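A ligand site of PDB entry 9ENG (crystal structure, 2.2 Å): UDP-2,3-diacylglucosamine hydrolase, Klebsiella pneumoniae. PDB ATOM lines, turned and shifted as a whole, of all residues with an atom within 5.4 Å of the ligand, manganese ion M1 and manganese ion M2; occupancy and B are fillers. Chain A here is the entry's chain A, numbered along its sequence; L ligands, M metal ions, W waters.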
ATOM      1  N   ASP A   8      10.669   8.475  23.577  1.00  0.00           N
ATOM      2  CA  ASP A   8      10.728   8.574  25.031  1.00  0.00           C
ATOM      3  C   ASP A   8       9.374   8.296  25.661  1.00  0.00           C
ATOM      4  O   ASP A   8       9.011   8.871  26.682  1.00  0.00           O
ATOM      5  CB  ASP A   8      11.329   9.919  25.438  1.00  0.00           C
ATOM      6  CG  ASP A   8      12.794  10.026  25.037  1.00  0.00           C
ATOM      7  OD1 ASP A   8      13.566   9.259  25.570  1.00  0.00           O
ATOM      8  OD2 ASP A   8      13.137  10.825  24.146  1.00  0.00           O
ATOM      9  N   HIS A  10       8.818   5.361  26.985  1.00  0.00           N
ATOM     10  CA  HIS A  10       9.185   4.490  28.104  1.00  0.00           C
ATOM     11  C   HIS A  10       8.040   3.593  28.535  1.00  0.00           C
ATOM     12  O   HIS A  10       7.657   3.566  29.701  1.00  0.00           O
ATOM     13  CB  HIS A  10       9.717   5.319  29.281  1.00  0.00           C
ATOM     14  CG  HIS A  10      11.007   6.006  28.987  1.00  0.00           C
ATOM     15  ND1 HIS A  10      12.251   5.520  29.323  1.00  0.00           N
ATOM     16  CD2 HIS A  10      11.230   7.153  28.328  1.00  0.00           C
ATOM     17  CE1 HIS A  10      13.185   6.353  28.900  1.00  0.00           C
ATOM     18  NE2 HIS A  10      12.580   7.364  28.308  1.00  0.00           N
ATOM     19  N   ASP A  41      13.582   4.827  22.913  1.00  0.00           N
ATOM     20  CA  ASP A  41      12.941   4.724  24.212  1.00  0.00           C
ATOM     21  C   ASP A  41      11.422   4.612  24.022  1.00  0.00           C
ATOM     22  O   ASP A  41      10.625   5.186  24.769  1.00  0.00           O
ATOM     23  CB  ASP A  41      13.323   5.894  25.123  1.00  0.00           C
ATOM     24  CG  ASP A  41      14.770   5.891  25.595  1.00  0.00           C
ATOM     25  OD1 ASP A  41      15.504   4.949  25.195  1.00  0.00           O
ATOM     26  OD2 ASP A  41      15.147   6.839  26.353  1.00  0.00           O
ATOM     27  N   GLU A  44      10.580   1.011  28.140  1.00  0.00           N
ATOM     28  CA  GLU A  44      11.352   1.316  29.337  1.00  0.00           C
ATOM     29  C   GLU A  44      12.555   0.362  29.461  1.00  0.00           C
ATOM     30  O   GLU A  44      13.553   0.705  30.086  1.00  0.00           O
ATOM     31  CB  GLU A  44      10.480   1.136  30.577  1.00  0.00           C
ATOM     32  CG  GLU A  44      11.197   1.389  31.907  1.00  0.00           C
ATOM     33  CD  GLU A  44      12.104   2.609  31.930  1.00  0.00           C
ATOM     34  OE1 GLU A  44      12.038   3.422  30.985  1.00  0.00           O
ATOM     35  OE2 GLU A  44      12.884   2.744  32.896  1.00  0.00           O
ATOM     36  N   ALA A  45      12.395  -0.834  28.905  1.00  0.00           N
ATOM     37  CA  ALA A  45      13.406  -1.874  28.942  1.00  0.00           C
ATOM     38  C   ALA A  45      13.110  -2.885  27.849  1.00  0.00           C
ATOM     39  O   ALA A  45      11.974  -2.999  27.374  1.00  0.00           O
ATOM     40  CB  ALA A  45      13.423  -2.522  30.306  1.00  0.00           C
ATOM     41  N   TRP A  46      14.156  -3.562  27.404  1.00  0.00           N
ATOM     42  CA  TRP A  46      14.016  -4.626  26.428  1.00  0.00           C
ATOM     43  C   TRP A  46      15.120  -5.650  26.679  1.00  0.00           C
ATOM     44  O   TRP A  46      16.284  -5.260  26.785  1.00  0.00           O
ATOM     45  CB  TRP A  46      14.144  -4.044  25.024  1.00  0.00           C
ATOM     46  CG  TRP A  46      13.559  -4.921  23.966  1.00  0.00           C
ATOM     47  CD1 TRP A  46      14.216  -5.792  23.149  1.00  0.00           C
ATOM     48  CD2 TRP A  46      12.186  -4.953  23.568  1.00  0.00           C
ATOM     49  NE1 TRP A  46      13.333  -6.380  22.275  1.00  0.00           N
ATOM     50  CE2 TRP A  46      12.077  -5.885  22.522  1.00  0.00           C
ATOM     51  CE3 TRP A  46      11.032  -4.292  24.022  1.00  0.00           C
ATOM     52  CZ2 TRP A  46      10.858  -6.177  21.906  1.00  0.00           C
ATOM     53  CZ3 TRP A  46       9.838  -4.556  23.389  1.00  0.00           C
ATOM     54  CH2 TRP A  46       9.752  -5.511  22.368  1.00  0.00           C
ATOM     55  N   ILE A  47      14.754  -6.937  26.757  1.00  0.00           N
ATOM     56  CA  ILE A  47      15.730  -7.990  26.950  1.00  0.00           C
ATOM     57  C   ILE A  47      15.716  -8.970  25.780  1.00  0.00           C
ATOM     58  O   ILE A  47      16.339 -10.006  25.882  1.00  0.00           O
ATOM     59  CB  ILE A  47      15.517  -8.712  28.286  1.00  0.00           C
ATOM     60  CG1 ILE A  47      14.120  -9.332  28.369  1.00  0.00           C
ATOM     61  CG2 ILE A  47      15.797  -7.780  29.447  1.00  0.00           C
ATOM     62  CD1 ILE A  47      14.044 -10.557  29.257  1.00  0.00           C
ATOM     63  N   GLY A  78      16.889   3.640  21.260  1.00  0.00           N
ATOM     64  CA  GLY A  78      17.389   4.433  22.360  1.00  0.00           C
ATOM     65  C   GLY A  78      18.310   3.606  23.257  1.00  0.00           C
ATOM     66  O   GLY A  78      18.626   2.476  22.928  1.00  0.00           O
ATOM     67  N   ASN A  79      18.730   4.219  24.359  1.00  0.00           N
ATOM     68  CA  ASN A  79      19.586   3.572  25.331  1.00  0.00           C
ATOM     69  C   ASN A  79      18.801   2.480  26.087  1.00  0.00           C
ATOM     70  O   ASN A  79      19.400   1.550  26.615  1.00  0.00           O
ATOM     71  CB  ASN A  79      20.193   4.607  26.288  1.00  0.00           C
ATOM     72  CG  ASN A  79      19.166   5.438  27.031  1.00  0.00           C
ATOM     73  OD1 ASN A  79      18.559   6.334  26.452  1.00  0.00           O
ATOM     74  ND2 ASN A  79      18.982   5.175  28.310  1.00  0.00           N
ATOM     75  N   ARG A  80      17.463   2.622  26.162  1.00  0.00           N
ATOM     76  CA  ARG A  80      16.652   1.703  26.944  1.00  0.00           C
ATOM     77  C   ARG A  80      16.346   0.456  26.122  1.00  0.00           C
ATOM     78  O   ARG A  80      16.254  -0.628  26.694  1.00  0.00           O
ATOM     79  CB  ARG A  80      15.333   2.300  27.450  1.00  0.00           C
ATOM     80  CG  ARG A  80      15.471   3.544  28.344  1.00  0.00           C
ATOM     81  CD  ARG A  80      16.256   3.402  29.639  1.00  0.00           C
ATOM     82  NE  ARG A  80      15.772   2.264  30.399  1.00  0.00           N
ATOM     83  CZ  ARG A  80      16.307   1.814  31.522  1.00  0.00           C
ATOM     84  NH1 ARG A  80      17.200   2.526  32.167  1.00  0.00           N
ATOM     85  NH2 ARG A  80      15.898   0.643  32.003  1.00  0.00           N
ATOM     86  N   ASP A  81      16.174   0.614  24.801  1.00  0.00           N
ATOM     87  CA  ASP A  81      15.601  -0.427  23.960  1.00  0.00           C
ATOM     88  C   ASP A  81      16.481  -0.744  22.739  1.00  0.00           C
ATOM     89  O   ASP A  81      15.972  -1.203  21.707  1.00  0.00           O
ATOM     90  CB  ASP A  81      14.167  -0.092  23.551  1.00  0.00           C
ATOM     91  CG  ASP A  81      13.923   1.320  23.037  1.00  0.00           C
ATOM     92  OD1 ASP A  81      14.904   2.100  22.843  1.00  0.00           O
ATOM     93  OD2 ASP A  81      12.756   1.619  22.790  1.00  0.00           O
ATOM     94  N   PHE A  82      17.807  -0.634  22.908  1.00  0.00           N
ATOM     95  CA  PHE A  82      18.739  -0.967  21.825  1.00  0.00           C
ATOM     96  C   PHE A  82      18.647  -2.433  21.382  1.00  0.00           C
ATOM     97  O   PHE A  82      19.136  -2.778  20.307  1.00  0.00           O
ATOM     98  CB  PHE A  82      20.178  -0.648  22.248  1.00  0.00           C
ATOM     99  CG  PHE A  82      20.616  -1.365  23.499  1.00  0.00           C
ATOM    100  CD1 PHE A  82      21.344  -2.538  23.433  1.00  0.00           C
ATOM    101  CD2 PHE A  82      20.314  -0.860  24.754  1.00  0.00           C
ATOM    102  CE1 PHE A  82      21.765  -3.172  24.589  1.00  0.00           C
ATOM    103  CE2 PHE A  82      20.732  -1.497  25.900  1.00  0.00           C
ATOM    104  CZ  PHE A  82      21.424  -2.676  25.813  1.00  0.00           C
ATOM    105  N   LEU A  83      18.034  -3.318  22.182  1.00  0.00           N
ATOM    106  CA  LEU A  83      17.982  -4.731  21.808  1.00  0.00           C
ATOM    107  C   LEU A  83      16.740  -5.013  20.973  1.00  0.00           C
ATOM    108  O   LEU A  83      16.549  -6.143  20.541  1.00  0.00           O
ATOM    109  CB  LEU A  83      17.974  -5.578  23.070  1.00  0.00           C
ATOM    110  CG  LEU A  83      19.313  -5.698  23.810  1.00  0.00           C
ATOM    111  CD1 LEU A  83      19.156  -6.550  25.064  1.00  0.00           C
ATOM    112  CD2 LEU A  83      20.387  -6.269  22.877  1.00  0.00           C
ATOM    113  N   HIS A 114      18.432   9.464  18.432  1.00  0.00           N
ATOM    114  CA  HIS A 114      17.800   9.357  19.730  1.00  0.00           C
ATOM    115  C   HIS A 114      18.232  10.539  20.593  1.00  0.00           C
ATOM    116  O   HIS A 114      17.431  11.085  21.352  1.00  0.00           O
ATOM    117  CB  HIS A 114      18.100   8.043  20.468  1.00  0.00           C
ATOM    118  CG  HIS A 114      17.512   8.016  21.846  1.00  0.00           C
ATOM    119  ND1 HIS A 114      16.144   8.050  21.993  1.00  0.00           N
ATOM    120  CD2 HIS A 114      18.026   7.964  23.080  1.00  0.00           C
ATOM    121  CE1 HIS A 114      15.854   8.021  23.292  1.00  0.00           C
ATOM    122  NE2 HIS A 114      16.973   7.955  23.974  1.00  0.00           N
ATOM    123  N   ASP A 116      21.211  10.374  22.603  1.00  0.00           N
ATOM    124  CA  ASP A 116      22.118   9.979  23.662  1.00  0.00           C
ATOM    125  C   ASP A 116      23.576  10.052  23.210  1.00  0.00           C
ATOM    126  O   ASP A 116      24.463  10.227  24.048  1.00  0.00           O
ATOM    127  CB  ASP A 116      21.788   8.580  24.204  1.00  0.00           C
ATOM    128  CG  ASP A 116      21.893   7.495  23.158  1.00  0.00           C
ATOM    129  OD1 ASP A 116      22.708   6.569  23.349  1.00  0.00           O
ATOM    130  OD2 ASP A 116      21.156   7.581  22.161  1.00  0.00           O
ATOM    131  N   ASP A 122      28.929  12.665  29.646  1.00  0.00           N
ATOM    132  CA  ASP A 122      28.705  11.526  30.511  1.00  0.00           C
ATOM    133  C   ASP A 122      29.673  10.425  30.121  1.00  0.00           C
ATOM    134  O   ASP A 122      29.303   9.465  29.442  1.00  0.00           O
ATOM    135  CB  ASP A 122      27.240  11.070  30.445  1.00  0.00           C
ATOM    136  CG  ASP A 122      26.838  10.161  31.591  1.00  0.00           C
ATOM    137  OD1 ASP A 122      27.749   9.657  32.319  1.00  0.00           O
ATOM    138  OD2 ASP A 122      25.613   9.986  31.777  1.00  0.00           O
ATOM    139  N   GLY A 124      30.731   7.970  31.631  1.00  0.00           N
ATOM    140  CA  GLY A 124      30.465   6.637  32.122  1.00  0.00           C
ATOM    141  C   GLY A 124      29.310   5.965  31.400  1.00  0.00           C
ATOM    142  O   GLY A 124      29.228   4.740  31.343  1.00  0.00           O
ATOM    143  N   TYR A 125      28.375   6.765  30.868  1.00  0.00           N
ATOM    144  CA  TYR A 125      27.360   6.204  29.993  1.00  0.00           C
ATOM    145  C   TYR A 125      27.996   5.763  28.680  1.00  0.00           C
ATOM    146  O   TYR A 125      27.555   4.791  28.077  1.00  0.00           O
ATOM    147  CB  TYR A 125      26.238   7.195  29.682  1.00  0.00           C
ATOM    148  CG  TYR A 125      25.365   6.733  28.537  1.00  0.00           C
ATOM    149  CD1 TYR A 125      24.435   5.722  28.711  1.00  0.00           C
ATOM    150  CD2 TYR A 125      25.523   7.254  27.260  1.00  0.00           C
ATOM    151  CE1 TYR A 125      23.650   5.272  27.673  1.00  0.00           C
ATOM    152  CE2 TYR A 125      24.754   6.812  26.204  1.00  0.00           C
ATOM    153  CZ  TYR A 125      23.819   5.812  26.419  1.00  0.00           C
ATOM    154  OH  TYR A 125      23.035   5.340  25.411  1.00  0.00           O
ATOM    155  N   PHE A 128      29.236   2.221  29.117  1.00  0.00           N
ATOM    156  CA  PHE A 128      28.107   1.320  29.051  1.00  0.00           C
ATOM    157  C   PHE A 128      27.643   1.130  27.606  1.00  0.00           C
ATOM    158  O   PHE A 128      27.372  -0.005  27.183  1.00  0.00           O
ATOM    159  CB  PHE A 128      26.979   1.876  29.926  1.00  0.00           C
ATOM    160  CG  PHE A 128      25.707   1.066  29.901  1.00  0.00           C
ATOM    161  CD1 PHE A 128      25.547  -0.034  30.737  1.00  0.00           C
ATOM    162  CD2 PHE A 128      24.665   1.406  29.038  1.00  0.00           C
ATOM    163  CE1 PHE A 128      24.368  -0.771  30.728  1.00  0.00           C
ATOM    164  CE2 PHE A 128      23.495   0.664  29.029  1.00  0.00           C
ATOM    165  CZ  PHE A 128      23.348  -0.432  29.860  1.00  0.00           C
ATOM    166  N   LYS A 131      29.989  -0.858  25.281  1.00  0.00           N
ATOM    167  CA  LYS A 131      29.961  -2.284  25.555  1.00  0.00           C
ATOM    168  C   LYS A 131      28.676  -2.912  25.033  1.00  0.00           C
ATOM    169  O   LYS A 131      28.773  -3.902  24.336  1.00  0.00           O
ATOM    170  CB  LYS A 131      30.242  -2.568  27.023  1.00  0.00           C
ATOM    171  CG  LYS A 131      31.717  -2.420  27.384  1.00  0.00           C
ATOM    172  CD  LYS A 131      31.967  -2.077  28.829  1.00  0.00           C
ATOM    173  CE  LYS A 131      33.241  -1.295  29.041  1.00  0.00           C
ATOM    174  NZ  LYS A 131      33.270  -0.696  30.392  1.00  0.00           N
ATOM    175  N   VAL A 132      27.495  -2.317  25.332  1.00  0.00           N
ATOM    176  CA  VAL A 132      26.237  -2.992  25.008  1.00  0.00           C
ATOM    177  C   VAL A 132      25.974  -2.936  23.496  1.00  0.00           C
ATOM    178  O   VAL A 132      25.034  -3.595  23.027  1.00  0.00           O
ATOM    179  CB  VAL A 132      25.042  -2.501  25.858  1.00  0.00           C
ATOM    180  CG1 VAL A 132      25.288  -2.659  27.349  1.00  0.00           C
ATOM    181  CG2 VAL A 132      24.602  -1.069  25.557  1.00  0.00           C
ATOM    182  N   ILE A 137      28.769  -9.028  22.629  1.00  0.00           N
ATOM    183  CA  ILE A 137      28.206  -8.846  23.962  1.00  0.00           C
ATOM    184  C   ILE A 137      26.674  -8.945  23.880  1.00  0.00           C
ATOM    185  O   ILE A 137      26.061  -9.503  24.770  1.00  0.00           O
ATOM    186  CB  ILE A 137      28.696  -7.534  24.605  1.00  0.00           C
ATOM    187  CG1 ILE A 137      30.217  -7.496  24.626  1.00  0.00           C
ATOM    188  CG2 ILE A 137      28.120  -7.337  26.001  1.00  0.00           C
ATOM    189  CD1 ILE A 137      30.783  -6.355  25.441  1.00  0.00           C
ATOM    190  N   GLN A 138      26.074  -8.493  22.772  1.00  0.00           N
ATOM    191  CA  GLN A 138      24.634  -8.605  22.586  1.00  0.00           C
ATOM    192  C   GLN A 138      24.216 -10.069  22.459  1.00  0.00           C
ATOM    193  O   GLN A 138      23.287 -10.508  23.133  1.00  0.00           O
ATOM    194  CB  GLN A 138      24.171  -7.808  21.375  1.00  0.00           C
ATOM    195  CG  GLN A 138      24.436  -6.314  21.536  1.00  0.00           C
ATOM    196  CD  GLN A 138      23.602  -5.513  20.574  1.00  0.00           C
ATOM    197  OE1 GLN A 138      22.935  -6.049  19.697  1.00  0.00           O
ATOM    198  NE2 GLN A 138      23.641  -4.201  20.760  1.00  0.00           N
ATOM    199  N   PHE A 141      24.346 -12.014  25.521  1.00  0.00           N
ATOM    200  CA  PHE A 141      23.296 -11.685  26.457  1.00  0.00           C
ATOM    201  C   PHE A 141      22.012 -12.384  26.039  1.00  0.00           C
ATOM    202  O   PHE A 141      21.279 -12.889  26.891  1.00  0.00           O
ATOM    203  CB  PHE A 141      23.038 -10.180  26.546  1.00  0.00           C
ATOM    204  CG  PHE A 141      21.871  -9.860  27.447  1.00  0.00           C
ATOM    205  CD1 PHE A 141      22.038  -9.787  28.809  1.00  0.00           C
ATOM    206  CD2 PHE A 141      20.592  -9.699  26.918  1.00  0.00           C
ATOM    207  CE1 PHE A 141      20.975  -9.478  29.646  1.00  0.00           C
ATOM    208  CE2 PHE A 141      19.523  -9.402  27.749  1.00  0.00           C
ATOM    209  CZ  PHE A 141      19.719  -9.294  29.113  1.00  0.00           C
ATOM    210  N   ILE A 152      19.086 -10.454  35.438  1.00  0.00           N
ATOM    211  CA  ILE A 152      20.183  -9.530  35.183  1.00  0.00           C
ATOM    212  C   ILE A 152      19.630  -8.114  35.123  1.00  0.00           C
ATOM    213  O   ILE A 152      20.219  -7.201  35.681  1.00  0.00           O
ATOM    214  CB  ILE A 152      20.989  -9.903  33.925  1.00  0.00           C
ATOM    215  CG1 ILE A 152      21.772 -11.203  34.095  1.00  0.00           C
ATOM    216  CG2 ILE A 152      21.921  -8.764  33.523  1.00  0.00           C
ATOM    217  CD1 ILE A 152      22.196 -11.863  32.797  1.00  0.00           C
ATOM    218  N   ALA A 153      18.472  -7.949  34.455  1.00  0.00           N
ATOM    219  CA  ALA A 153      17.839  -6.640  34.301  1.00  0.00           C
ATOM    220  C   ALA A 153      17.451  -6.046  35.673  1.00  0.00           C
ATOM    221  O   ALA A 153      17.800  -4.906  35.965  1.00  0.00           O
ATOM    222  CB  ALA A 153      16.637  -6.749  33.388  1.00  0.00           C
ATOM    223  N   MET A 156      20.011  -4.791  37.931  1.00  0.00           N
ATOM    224  CA  MET A 156      20.632  -3.595  37.391  1.00  0.00           C
ATOM    225  C   MET A 156      20.021  -2.333  38.010  1.00  0.00           C
ATOM    226  O   MET A 156      20.533  -1.239  37.789  1.00  0.00           O
ATOM    227  CB  MET A 156      20.493  -3.535  35.860  1.00  0.00           C
ATOM    228  CG  MET A 156      21.511  -4.407  35.124  1.00  0.00           C
ATOM    229  SD  MET A 156      21.958  -3.757  33.488  1.00  0.00           S
ATOM    230  CE  MET A 156      22.849  -5.148  32.790  1.00  0.00           C
ATOM    231  N   GLU A 170      18.470  11.628  36.892  1.00  0.00           N
ATOM    232  CA  GLU A 170      18.727  12.933  36.216  1.00  0.00           C
ATOM    233  C   GLU A 170      19.603  12.699  34.986  1.00  0.00           C
ATOM    234  O   GLU A 170      20.723  12.223  35.104  1.00  0.00           O
ATOM    235  CB  GLU A 170      19.382  13.907  37.197  1.00  0.00           C
ATOM    236  CG  GLU A 170      18.728  13.884  38.567  1.00  0.00           C
ATOM    237  CD  GLU A 170      18.902  15.158  39.386  1.00  0.00           C
ATOM    238  OE1 GLU A 170      20.065  15.564  39.595  1.00  0.00           O
ATOM    239  OE2 GLU A 170      17.878  15.724  39.803  1.00  0.00           O
ATOM    240  N   ILE A 171      19.064  13.031  33.823  1.00  0.00           N
ATOM    241  CA  ILE A 171      19.668  12.706  32.537  1.00  0.00           C
ATOM    242  C   ILE A 171      20.552  13.862  32.074  1.00  0.00           C
ATOM    243  O   ILE A 171      20.073  14.970  31.843  1.00  0.00           O
ATOM    244  CB  ILE A 171      18.557  12.385  31.511  1.00  0.00           C
ATOM    245  CG1 ILE A 171      17.695  11.204  31.969  1.00  0.00           C
ATOM    246  CG2 ILE A 171      19.135  12.167  30.123  1.00  0.00           C
ATOM    247  CD1 ILE A 171      16.496  10.967  31.073  1.00  0.00           C
ATOM    248  N   MET A 172      21.843  13.567  31.894  1.00  0.00           N
ATOM    249  CA  MET A 172      22.822  14.497  31.345  1.00  0.00           C
ATOM    250  C   MET A 172      22.319  15.045  30.011  1.00  0.00           C
ATOM    251  O   MET A 172      21.961  14.252  29.143  1.00  0.00           O
ATOM    252  CB  MET A 172      24.142  13.729  31.104  1.00  0.00           C
ATOM    253  CG  MET A 172      25.306  14.595  30.702  1.00  0.00           C
ATOM    254  SD  MET A 172      25.911  15.487  32.146  1.00  0.00           S
ATOM    255  CE  MET A 172      27.096  14.311  32.802  1.00  0.00           C
ATOM    256  N   HIS A 195      15.642  11.770  24.153  1.00  0.00           N
ATOM    257  CA  HIS A 195      16.598  11.253  25.140  1.00  0.00           C
ATOM    258  C   HIS A 195      16.759  12.167  26.346  1.00  0.00           C
ATOM    259  O   HIS A 195      16.829  11.662  27.465  1.00  0.00           O
ATOM    260  CB  HIS A 195      17.989  10.958  24.552  1.00  0.00           C
ATOM    261  CG  HIS A 195      18.902  10.461  25.606  1.00  0.00           C
ATOM    262  ND1 HIS A 195      18.695   9.299  26.324  1.00  0.00           N
ATOM    263  CD2 HIS A 195      19.989  11.054  26.134  1.00  0.00           C
ATOM    264  CE1 HIS A 195      19.664   9.190  27.233  1.00  0.00           C
ATOM    265  NE2 HIS A 195      20.462  10.244  27.138  1.00  0.00           N
ATOM    266  N   HIS A 197      14.832  14.474  27.535  1.00  0.00           N
ATOM    267  CA  HIS A 197      13.563  14.671  28.243  1.00  0.00           C
ATOM    268  C   HIS A 197      13.277  16.154  28.524  1.00  0.00           C
ATOM    269  O   HIS A 197      12.374  16.450  29.296  1.00  0.00           O
ATOM    270  CB  HIS A 197      13.492  13.811  29.514  1.00  0.00           C
ATOM    271  CG  HIS A 197      13.428  12.343  29.263  1.00  0.00           C
ATOM    272  ND1 HIS A 197      13.137  11.419  30.246  1.00  0.00           N
ATOM    273  CD2 HIS A 197      13.555  11.641  28.126  1.00  0.00           C
ATOM    274  CE1 HIS A 197      13.084  10.214  29.702  1.00  0.00           C
ATOM    275  NE2 HIS A 197      13.317  10.332  28.403  1.00  0.00           N
HETATM  276  C1  LIG L   1      24.075  -7.084  29.250  1.00  0.00           C
HETATM  277  C2  LIG L   1      22.864  -6.487  29.643  1.00  0.00           C
HETATM  278  C3  LIG L   1      22.046  -5.920  28.672  1.00  0.00           C
HETATM  279  C4  LIG L   1      22.514  -5.871  27.390  1.00  0.00           C
HETATM  280  C5  LIG L   1      23.725  -6.450  27.055  1.00  0.00           C
HETATM  281  C6  LIG L   1      24.537  -7.071  27.962  1.00  0.00           C
HETATM  282  N1  LIG L   1      20.830  -5.263  29.010  1.00  0.00           N
HETATM  283  C7  LIG L   1      19.851  -5.099  27.981  1.00  0.00           C
HETATM  284  C8  LIG L   1      18.965  -3.925  28.379  1.00  0.00           C
HETATM  285  C9  LIG L   1      20.186  -5.811  30.200  1.00  0.00           C
HETATM  286  C10 LIG L   1      19.209  -4.738  30.769  1.00  0.00           C
HETATM  287  N2  LIG L   1      18.257  -4.185  29.690  1.00  0.00           N
HETATM  288  S1  LIG L   1      17.237  -2.971  30.180  1.00  0.00           S
HETATM  289  C11 LIG L   1      18.235  -1.615  30.557  1.00  0.00           C
HETATM  290  O1  LIG L   1      16.399  -2.635  29.073  1.00  0.00           O
HETATM  291  O2  LIG L   1      16.633  -3.396  31.411  1.00  0.00           O
HETATM  292  C12 LIG L   1      18.632  -1.415  31.861  1.00  0.00           C
HETATM  293  C13 LIG L   1      19.477  -0.381  32.181  1.00  0.00           C
HETATM  294  C14 LIG L   1      19.929   0.462  31.193  1.00  0.00           C
HETATM  295  C15 LIG L   1      18.715  -0.781  29.555  1.00  0.00           C
HETATM  296  C16 LIG L   1      19.578   0.245  29.875  1.00  0.00           C
HETATM  297  N3  LIG L   1      20.817   1.469  31.547  1.00  0.00           N
HETATM  298  C17 LIG L   1      20.889   2.651  30.885  1.00  0.00           C
HETATM  299  O3  LIG L   1      20.148   2.883  29.930  1.00  0.00           O
HETATM  300  C18 LIG L   1      21.930   3.666  31.355  1.00  0.00           C
HETATM  301  C19 LIG L   1      23.229   3.223  31.661  1.00  0.00           C
HETATM  302  C20 LIG L   1      24.198   4.119  32.117  1.00  0.00           C
HETATM  303  C21 LIG L   1      23.892   5.456  32.285  1.00  0.00           C
HETATM  304  C22 LIG L   1      22.604   5.919  31.979  1.00  0.00           C
HETATM  305  C23 LIG L   1      21.614   5.027  31.537  1.00  0.00           C
HETATM  306  N4  LIG L   1      22.312   7.327  32.181  1.00  0.00           N
HETATM  307  S2  LIG L   1      21.730   8.290  30.965  1.00  0.00           S
HETATM  308  C24 LIG L   1      23.073   9.007  30.032  1.00  0.00           C
HETATM  309  O4  LIG L   1      20.943   7.469  30.085  1.00  0.00           O
HETATM  310  O5  LIG L   1      21.098   9.398  31.595  1.00  0.00           O
HETATM  311 CL1  LIG L   1      24.220  -6.416  25.432  1.00  0.00          CL
HETATM  312 CL2  LIG L   1      25.052  -7.904  30.406  1.00  0.00          CL
HETATM  313 MN    MN M   1      17.037   7.840  26.216  1.00  0.00          MN
HETATM  314 MN    MN M   2      14.201   8.520  27.423  1.00  0.00          MN
HETATM  315  O   HOH W   1      16.221   9.149  27.787  1.00  0.00           O
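Manganese ion M2 is bound by the side-chain carboxylate (OD1) of Asp 8 (2.1 Å).
Manganese ion M2 is bound by water W1 (2.1 Å).
NE2 of His 10 binds manganese ion M2 (2.2 Å).
Manganese ion M2 is bound by OD2 of Asp 41, 2.2 Å away.
NE2 of His 197 is bound to manganese ion M2 (2.2 Å).
Manganese ion M2 has five donor atoms within binding distance.
The side-chain carboxylate (OD2) of Asp 8 lies within hydrogen-bond range of the backbone NH (N) of His 195.
The side-chain carboxylate (OD1) of Asp 41 is in hydrogen-bond range of the backbone NH (N) of Arg 80 (3.2 Å).
N of Asp 41 is in hydrogen-bond range of OD1 of Asp 81.
The side-chain carboxylate (OE1) of Glu 44 is in hydrogen-bond range of a ring nitrogen (ND1) of His 10 (2.7 Å).
The guanidinium group (NH2) of Arg 80 lies within salt-bridge range of the side-chain carboxylate (OE2) of Glu 44 (3.8 Å).
The backbone NH of Tyr 125 is in hydrogen-bond range of the side-chain carboxylate of Asp 122, 3.3 Å away.
The side-chain hydroxyl (OH) of Tyr 125 sits at hydrogen-bond distance from the side-chain carboxylate (OD1) of Asp 116.
The side-chain amide nitrogen of Gln 138 is in hydrogen-bond range of the backbone carbonyl oxygen of Val 132, at 2.7 Å.
The backbone carbonyl oxygen (O) of Arg 80 lies close to an oxygen (O1) of the ligand, at 3.1 Å.
Residues that only touch the ligand: Ala 45, Asp 122, Leu 83, Phe 141, Met 156, Phe 128, Tyr 125, Phe 82, Gln 138, Ile 137, Ile 171, Val 132 and Ala 153.
Hydrophobic or aromatic side chains within 4 Å of the ligand: Ala 45, Phe 82, Leu 83, Tyr 125, Phe 128, Phe 141, Ala 153, Met 156, Ile 171 and His 195.
Of the 32 residues printed, 17 come within 4 Å of the ligand.
The nearest printed residue that does not touch the ligand is Met 172 (4.2 Å).
Within 4 Å of manganese ion M1: Asp 8, Asp 41, Asn 79, His 114 and His 195.
The nearest printed residue that does not touch manganese ion M1 is His 10 (4.9 Å).
Of the 32 residues printed, 4 come within 4 Å of manganese ion M2.
The nearest printed residue that does not touch manganese ion M2 is His 195 (4.1 Å).
ND2 of Asn 79 is in hydrogen-bond range of O3 of the ligand, 3.0 Å away.
An oxygen (O1) of the ligand sits at hydrogen-bond distance from the backbone NH (N) of Trp 46, 2.9 Å away.
Manganese ion M1 is bound by the side-chain carboxylate of Asp 41 (2.1 Å), the side-chain amide oxygen of Asn 79 (2.2 Å), water W1 (2.2 Å), a ring nitrogen (ND1) of His 195 (2.2 Å) and a ring nitrogen (NE2) of His 114 (2.2 Å).
Manganese ion M1 has five donor atoms within binding distance.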
